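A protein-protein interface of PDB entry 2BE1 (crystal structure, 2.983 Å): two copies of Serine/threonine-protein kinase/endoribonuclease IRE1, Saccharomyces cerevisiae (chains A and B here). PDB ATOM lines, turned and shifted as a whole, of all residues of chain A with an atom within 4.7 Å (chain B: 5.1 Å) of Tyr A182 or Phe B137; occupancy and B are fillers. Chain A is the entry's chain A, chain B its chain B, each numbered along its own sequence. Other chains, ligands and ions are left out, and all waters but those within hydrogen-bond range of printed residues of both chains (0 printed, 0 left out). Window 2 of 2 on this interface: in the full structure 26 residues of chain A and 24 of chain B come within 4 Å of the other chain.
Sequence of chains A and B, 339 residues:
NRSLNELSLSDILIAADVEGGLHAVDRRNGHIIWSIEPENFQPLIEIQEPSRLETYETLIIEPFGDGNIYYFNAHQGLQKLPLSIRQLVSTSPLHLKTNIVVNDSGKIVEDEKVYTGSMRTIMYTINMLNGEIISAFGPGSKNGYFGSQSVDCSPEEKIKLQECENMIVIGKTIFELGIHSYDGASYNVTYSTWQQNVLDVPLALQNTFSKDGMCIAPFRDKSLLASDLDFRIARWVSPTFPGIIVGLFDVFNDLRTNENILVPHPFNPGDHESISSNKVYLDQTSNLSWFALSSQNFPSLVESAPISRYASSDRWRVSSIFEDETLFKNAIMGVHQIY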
ATOM      1  N   ASP A 111     -17.582   6.464 -18.926  1.00  0.00           N
ATOM      2  CA  ASP A 111     -17.461   5.223 -19.732  1.00  0.00           C
ATOM      3  C   ASP A 111     -18.757   4.504 -20.122  1.00  0.00           C
ATOM      4  O   ASP A 111     -19.750   4.583 -19.408  1.00  0.00           O
ATOM      5  CB  ASP A 111     -16.517   4.203 -19.066  1.00  0.00           C
ATOM      6  CG  ASP A 111     -16.194   2.998 -19.984  1.00  0.00           C
ATOM      7  OD1 ASP A 111     -16.038   1.879 -19.439  1.00  0.00           O
ATOM      8  OD2 ASP A 111     -16.117   3.163 -21.241  1.00  0.00           O
ATOM      9  N   GLU A 112     -18.701   3.770 -21.239  1.00  0.00           N
ATOM     10  CA  GLU A 112     -19.794   2.916 -21.681  1.00  0.00           C
ATOM     11  C   GLU A 112     -19.558   1.378 -21.674  1.00  0.00           C
ATOM     12  O   GLU A 112     -18.535   0.884 -22.148  1.00  0.00           O
ATOM     13  CB  GLU A 112     -20.261   3.384 -23.042  1.00  0.00           C
ATOM     14  CG  GLU A 112     -19.165   3.651 -23.985  1.00  0.00           C
ATOM     15  CD  GLU A 112     -19.665   3.560 -25.382  1.00  0.00           C
ATOM     16  OE1 GLU A 112     -19.988   2.461 -25.830  1.00  0.00           O
ATOM     17  OE2 GLU A 112     -19.774   4.585 -26.052  1.00  0.00           O
ATOM     18  N   VAL A 114     -21.702  -2.547 -22.548  1.00  0.00           N
ATOM     19  CA  VAL A 114     -22.780  -3.240 -23.263  1.00  0.00           C
ATOM     20  C   VAL A 114     -23.002  -4.668 -22.725  1.00  0.00           C
ATOM     21  O   VAL A 114     -22.066  -5.466 -22.666  1.00  0.00           O
ATOM     22  CB  VAL A 114     -22.574  -3.201 -24.819  1.00  0.00           C
ATOM     23  CG1 VAL A 114     -21.296  -3.805 -25.236  1.00  0.00           C
ATOM     24  CG2 VAL A 114     -23.651  -3.954 -25.503  1.00  0.00           C
ATOM     25  N   THR A 116     -24.595  -8.216 -22.988  1.00  0.00           N
ATOM     26  CA  THR A 116     -25.200  -9.213 -23.818  1.00  0.00           C
ATOM     27  C   THR A 116     -25.380 -10.456 -23.009  1.00  0.00           C
ATOM     28  O   THR A 116     -24.529 -10.849 -22.228  1.00  0.00           O
ATOM     29  CB  THR A 116     -24.375  -9.549 -25.015  1.00  0.00           C
ATOM     30  OG1 THR A 116     -23.139 -10.111 -24.595  1.00  0.00           O
ATOM     31  CG2 THR A 116     -24.100  -8.349 -25.731  1.00  0.00           C
ATOM     32  N   HIS A 180     -19.232  -6.010 -21.585  1.00  0.00           N
ATOM     33  CA  HIS A 180     -18.153  -5.506 -22.480  1.00  0.00           C
ATOM     34  C   HIS A 180     -17.947  -4.035 -22.434  1.00  0.00           C
ATOM     35  O   HIS A 180     -18.566  -3.287 -23.141  1.00  0.00           O
ATOM     36  CB  HIS A 180     -18.336  -5.940 -23.928  1.00  0.00           C
ATOM     37  CG  HIS A 180     -18.276  -7.427 -24.107  1.00  0.00           C
ATOM     38  ND1 HIS A 180     -17.534  -8.253 -23.266  1.00  0.00           N
ATOM     39  CD2 HIS A 180     -18.873  -8.247 -25.015  1.00  0.00           C
ATOM     40  CE1 HIS A 180     -17.671  -9.512 -23.656  1.00  0.00           C
ATOM     41  NE2 HIS A 180     -18.480  -9.536 -24.714  1.00  0.00           N
ATOM     42  N   SER A 181     -17.037  -3.648 -21.568  1.00  0.00           N
ATOM     43  CA  SER A 181     -16.759  -2.265 -21.290  1.00  0.00           C
ATOM     44  C   SER A 181     -15.623  -1.862 -22.212  1.00  0.00           C
ATOM     45  O   SER A 181     -14.673  -2.620 -22.393  1.00  0.00           O
ATOM     46  CB  SER A 181     -16.360  -2.135 -19.814  1.00  0.00           C
ATOM     47  OG  SER A 181     -16.227  -0.782 -19.407  1.00  0.00           O
ATOM     48  N   TYR A 182     -15.726  -0.672 -22.791  1.00  0.00           N
ATOM     49  CA  TYR A 182     -14.824  -0.250 -23.869  1.00  0.00           C
ATOM     50  C   TYR A 182     -13.494   0.278 -23.425  1.00  0.00           C
ATOM     51  O   TYR A 182     -12.542   0.274 -24.197  1.00  0.00           O
ATOM     52  CB  TYR A 182     -15.471   0.805 -24.724  1.00  0.00           C
ATOM     53  CG  TYR A 182     -16.528   0.231 -25.624  1.00  0.00           C
ATOM     54  CD1 TYR A 182     -17.817  -0.037 -25.134  1.00  0.00           C
ATOM     55  CD2 TYR A 182     -16.250  -0.051 -26.972  1.00  0.00           C
ATOM     56  CE1 TYR A 182     -18.796  -0.557 -25.956  1.00  0.00           C
ATOM     57  CE2 TYR A 182     -17.227  -0.562 -27.806  1.00  0.00           C
ATOM     58  CZ  TYR A 182     -18.497  -0.811 -27.284  1.00  0.00           C
ATOM     59  OH  TYR A 182     -19.490  -1.314 -28.086  1.00  0.00           O
ATOM     60  N   ASP A 183     -13.435   0.765 -22.194  1.00  0.00           N
ATOM     61  CA  ASP A 183     -12.167   1.044 -21.568  1.00  0.00           C
ATOM     62  C   ASP A 183     -11.397  -0.276 -21.477  1.00  0.00           C
ATOM     63  O   ASP A 183     -10.197  -0.267 -21.473  1.00  0.00           O
ATOM     64  CB  ASP A 183     -12.372   1.672 -20.192  1.00  0.00           C
ATOM     65  CG  ASP A 183     -12.645   0.635 -19.110  1.00  0.00           C
ATOM     66  OD1 ASP A 183     -13.805   0.179 -18.951  1.00  0.00           O
ATOM     67  OD2 ASP A 183     -11.683   0.269 -18.408  1.00  0.00           O
ATOM     68  N   GLY A 184     -12.087  -1.411 -21.429  1.00  0.00           N
ATOM     69  CA  GLY A 184     -11.418  -2.710 -21.384  1.00  0.00           C
ATOM     70  C   GLY A 184     -11.763  -3.585 -20.190  1.00  0.00           C
ATOM     71  O   GLY A 184     -11.587  -4.793 -20.293  1.00  0.00           O
ATOM     72  N   THR B 121     -28.699 -13.127 -26.619  1.00  0.00           N
ATOM     73  CA  THR B 121     -28.785 -11.714 -26.893  1.00  0.00           C
ATOM     74  C   THR B 121     -27.505 -11.274 -27.650  1.00  0.00           C
ATOM     75  O   THR B 121     -26.452 -11.873 -27.450  1.00  0.00           O
ATOM     76  CB  THR B 121     -28.981 -11.045 -25.540  1.00  0.00           C
ATOM     77  OG1 THR B 121     -30.322 -10.585 -25.472  1.00  0.00           O
ATOM     78  CG2 THR B 121     -28.080  -9.908 -25.363  1.00  0.00           C
ATOM     79  N   ILE B 122     -27.606 -10.274 -28.526  1.00  0.00           N
ATOM     80  CA  ILE B 122     -26.479  -9.717 -29.289  1.00  0.00           C
ATOM     81  C   ILE B 122     -26.671  -8.215 -29.528  1.00  0.00           C
ATOM     82  O   ILE B 122     -27.817  -7.725 -29.622  1.00  0.00           O
ATOM     83  CB  ILE B 122     -26.387 -10.353 -30.664  1.00  0.00           C
ATOM     84  CG1 ILE B 122     -25.514 -11.593 -30.619  1.00  0.00           C
ATOM     85  CG2 ILE B 122     -25.761  -9.395 -31.666  1.00  0.00           C
ATOM     86  CD1 ILE B 122     -24.990 -12.050 -32.039  1.00  0.00           C
ATOM     87  N   MET B 123     -25.572  -7.476 -29.669  1.00  0.00           N
ATOM     88  CA  MET B 123     -25.664  -6.050 -30.044  1.00  0.00           C
ATOM     89  C   MET B 123     -24.731  -5.766 -31.221  1.00  0.00           C
ATOM     90  O   MET B 123     -23.610  -6.297 -31.251  1.00  0.00           O
ATOM     91  CB  MET B 123     -25.290  -5.157 -28.864  1.00  0.00           C
ATOM     92  CG  MET B 123     -25.946  -3.825 -28.920  1.00  0.00           C
ATOM     93  SD  MET B 123     -27.197  -3.704 -27.636  1.00  0.00           S
ATOM     94  CE  MET B 123     -28.186  -2.343 -28.264  1.00  0.00           C
ATOM     95  N   TYR B 124     -25.183  -4.964 -32.190  1.00  0.00           N
ATOM     96  CA  TYR B 124     -24.315  -4.546 -33.272  1.00  0.00           C
ATOM     97  C   TYR B 124     -24.316  -3.083 -33.208  1.00  0.00           C
ATOM     98  O   TYR B 124     -25.339  -2.514 -32.847  1.00  0.00           O
ATOM     99  CB  TYR B 124     -24.903  -4.915 -34.603  1.00  0.00           C
ATOM    100  CG  TYR B 124     -24.975  -6.382 -34.827  1.00  0.00           C
ATOM    101  CD1 TYR B 124     -26.125  -7.072 -34.522  1.00  0.00           C
ATOM    102  CD2 TYR B 124     -23.881  -7.094 -35.343  1.00  0.00           C
ATOM    103  CE1 TYR B 124     -26.209  -8.440 -34.698  1.00  0.00           C
ATOM    104  CE2 TYR B 124     -23.932  -8.490 -35.529  1.00  0.00           C
ATOM    105  CZ  TYR B 124     -25.115  -9.163 -35.188  1.00  0.00           C
ATOM    106  OH  TYR B 124     -25.262 -10.549 -35.325  1.00  0.00           O
ATOM    107  N   THR B 125     -23.197  -2.457 -33.548  1.00  0.00           N
ATOM    108  CA  THR B 125     -23.237  -1.040 -33.902  1.00  0.00           C
ATOM    109  C   THR B 125     -22.819  -0.879 -35.352  1.00  0.00           C
ATOM    110  O   THR B 125     -21.800  -1.407 -35.809  1.00  0.00           O
ATOM    111  CB  THR B 125     -22.325  -0.194 -33.078  1.00  0.00           C
ATOM    112  OG1 THR B 125     -20.996  -0.585 -33.393  1.00  0.00           O
ATOM    113  CG2 THR B 125     -22.583  -0.370 -31.583  1.00  0.00           C
ATOM    114  N   SER B 135     -18.951  -2.758 -34.928  1.00  0.00           N
ATOM    115  CA  SER B 135     -18.572  -3.758 -33.938  1.00  0.00           C
ATOM    116  C   SER B 135     -19.792  -4.576 -33.588  1.00  0.00           C
ATOM    117  O   SER B 135     -20.937  -4.081 -33.669  1.00  0.00           O
ATOM    118  CB  SER B 135     -17.997  -3.115 -32.692  1.00  0.00           C
ATOM    119  OG  SER B 135     -19.001  -2.545 -31.889  1.00  0.00           O
ATOM    120  N   ALA B 136     -19.548  -5.831 -33.223  1.00  0.00           N
ATOM    121  CA  ALA B 136     -20.609  -6.774 -32.944  1.00  0.00           C
ATOM    122  C   ALA B 136     -20.386  -7.328 -31.571  1.00  0.00           C
ATOM    123  O   ALA B 136     -19.313  -7.784 -31.268  1.00  0.00           O
ATOM    124  CB  ALA B 136     -20.559  -7.866 -33.932  1.00  0.00           C
ATOM    125  N   PHE B 137     -21.403  -7.321 -30.734  1.00  0.00           N
ATOM    126  CA  PHE B 137     -21.212  -7.838 -29.406  1.00  0.00           C
ATOM    127  C   PHE B 137     -22.118  -8.968 -28.956  1.00  0.00           C
ATOM    128  O   PHE B 137     -23.258  -9.099 -29.374  1.00  0.00           O
ATOM    129  CB  PHE B 137     -21.245  -6.686 -28.429  1.00  0.00           C
ATOM    130  CG  PHE B 137     -19.969  -5.938 -28.390  1.00  0.00           C
ATOM    131  CD1 PHE B 137     -19.900  -4.656 -28.899  1.00  0.00           C
ATOM    132  CD2 PHE B 137     -18.780  -6.554 -27.877  1.00  0.00           C
ATOM    133  CE1 PHE B 137     -18.668  -3.967 -28.888  1.00  0.00           C
ATOM    134  CE2 PHE B 137     -17.528  -5.870 -27.843  1.00  0.00           C
ATOM    135  CZ  PHE B 137     -17.473  -4.576 -28.345  1.00  0.00           C
ATOM    136  N   GLY B 138     -21.590  -9.762 -28.048  1.00  0.00           N
ATOM    137  CA  GLY B 138     -22.367 -10.793 -27.400  1.00  0.00           C
ATOM    138  C   GLY B 138     -22.054 -12.089 -28.088  1.00  0.00           C
ATOM    139  O   GLY B 138     -21.479 -12.020 -29.191  1.00  0.00           O
ATOM    140  N   PRO B 139     -22.387 -13.255 -27.433  1.00  0.00           N
ATOM    141  CA  PRO B 139     -22.420 -14.633 -27.936  1.00  0.00           C
ATOM    142  C   PRO B 139     -22.518 -14.780 -29.462  1.00  0.00           C
ATOM    143  O   PRO B 139     -23.241 -15.663 -29.958  1.00  0.00           O
ATOM    144  CB  PRO B 139     -23.685 -15.147 -27.280  1.00  0.00           C
ATOM    145  CG  PRO B 139     -23.624 -14.506 -25.889  1.00  0.00           C
ATOM    146  CD  PRO B 139     -22.774 -13.256 -26.003  1.00  0.00           C
ATOM    147  N   SER B 141     -19.877 -12.168 -32.067  1.00  0.00           N
ATOM    148  CA  SER B 141     -18.423 -12.048 -32.416  1.00  0.00           C
ATOM    149  C   SER B 141     -17.743 -10.739 -31.996  1.00  0.00           C
ATOM    150  O   SER B 141     -17.607  -9.821 -32.821  1.00  0.00           O
ATOM    151  CB  SER B 141     -18.176 -12.288 -33.908  1.00  0.00           C
ATOM    152  OG  SER B 141     -16.835 -11.985 -34.222  1.00  0.00           O
ATOM    153  N   LYS B 142     -17.258 -10.677 -30.754  1.00  0.00           N
ATOM    154  CA  LYS B 142     -16.999  -9.386 -30.083  1.00  0.00           C
ATOM    155  C   LYS B 142     -15.838  -8.502 -30.630  1.00  0.00           C
ATOM    156  O   LYS B 142     -14.713  -8.583 -30.160  1.00  0.00           O
ATOM    157  CB  LYS B 142     -16.933  -9.578 -28.557  1.00  0.00           C
ATOM    158  CG  LYS B 142     -18.171 -10.248 -27.925  1.00  0.00           C
ATOM    159  CD  LYS B 142     -18.155 -11.774 -28.078  1.00  0.00           C
ATOM    160  CE  LYS B 142     -18.720 -12.492 -26.849  1.00  0.00           C
ATOM    161  NZ  LYS B 142     -18.956 -13.952 -27.110  1.00  0.00           N
ATOM    162  N   ASN B 143     -16.148  -7.663 -31.627  1.00  0.00           N
ATOM    163  CA  ASN B 143     -15.204  -6.723 -32.268  1.00  0.00           C
ATOM    164  C   ASN B 143     -15.060  -5.396 -31.454  1.00  0.00           C
ATOM    165  O   ASN B 143     -15.568  -5.330 -30.315  1.00  0.00           O
ATOM    166  CB  ASN B 143     -15.647  -6.467 -33.724  1.00  0.00           C
ATOM    167  CG  ASN B 143     -14.624  -5.652 -34.545  1.00  0.00           C
ATOM    168  OD1 ASN B 143     -14.952  -5.169 -35.633  1.00  0.00           O
ATOM    169  ND2 ASN B 143     -13.396  -5.505 -34.036  1.00  0.00           N
ATOM    170  N   GLY B 144     -14.366  -4.374 -32.009  1.00  0.00           N
ATOM    171  CA  GLY B 144     -14.230  -3.037 -31.383  1.00  0.00           C
ATOM    172  C   GLY B 144     -14.132  -1.939 -32.426  1.00  0.00           C
ATOM    173  O   GLY B 144     -15.082  -1.193 -32.658  1.00  0.00           O
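Of the 14 printed residues of chain B, 6 touch a printed residue of chain A.
Hydrophobic or aromatic side chains of chain B that line the printed part of chain A: Met B123, Phe B137 and Pro B139.
Among the printed residues, 8 pairs touch across the chains.
Among the printed residues, no Asp or Glu carboxylate lies within 4 Å of a Lys or Arg side-chain nitrogen of the other chain.
The backbone carbonyl oxygen (O) of Glu A112 sits close to the backbone NH (N) of Tyr A182 (3.3 Å).
The backbone NH (N) of His A180 sits at hydrogen-bond distance from the backbone carbonyl oxygen (O) of Val A114 (3.1 Å).
The backbone carbonyl oxygen (O) of Met B123 is in hydrogen-bond range of the backbone NH (N) of Phe B137, at 2.5 Å.
Glu A112 touches none of the printed residues of chain B.
Of the printed residues of chain B, His A180 touches Phe B137 (3.3 Å) and Lys B142 (3.3 Å).
Of the printed residues of chain B, Tyr A182 touches Phe B137 (2.9 Å).
Thr B125 touches none of the printed residues of chain A.
Of the printed residues of chain A, Phe B137 touches Thr A116 (3.8 Å), His A180 (3.3 Å) and Tyr A182 (2.9 Å).
Of the printed residues of chain A, Lys B142 touches His A180.
The nearest residue of chain B that does not touch Tyr A182 is Ser B135 (4.03 Å).
The nearest printed residue of chain A that does not touch Phe B137 is Val A114 (4.01 Å).
Val A114 touches Met B123 (CG2 to CB, 3.9 Å).
Thr A116 touches Thr B121.
Thr A116 touches Phe B137.
Thr A116 touches Gly B138 (OG1 to CA, 3.0 Å).
Thr A116 touches Pro B139.
CD2 of His A180 touches CD2 of Phe B137, 3.3 Å away.
His A180 touches Lys B142.
Phe B137 touches Tyr A182.
No position is printed for both chains.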
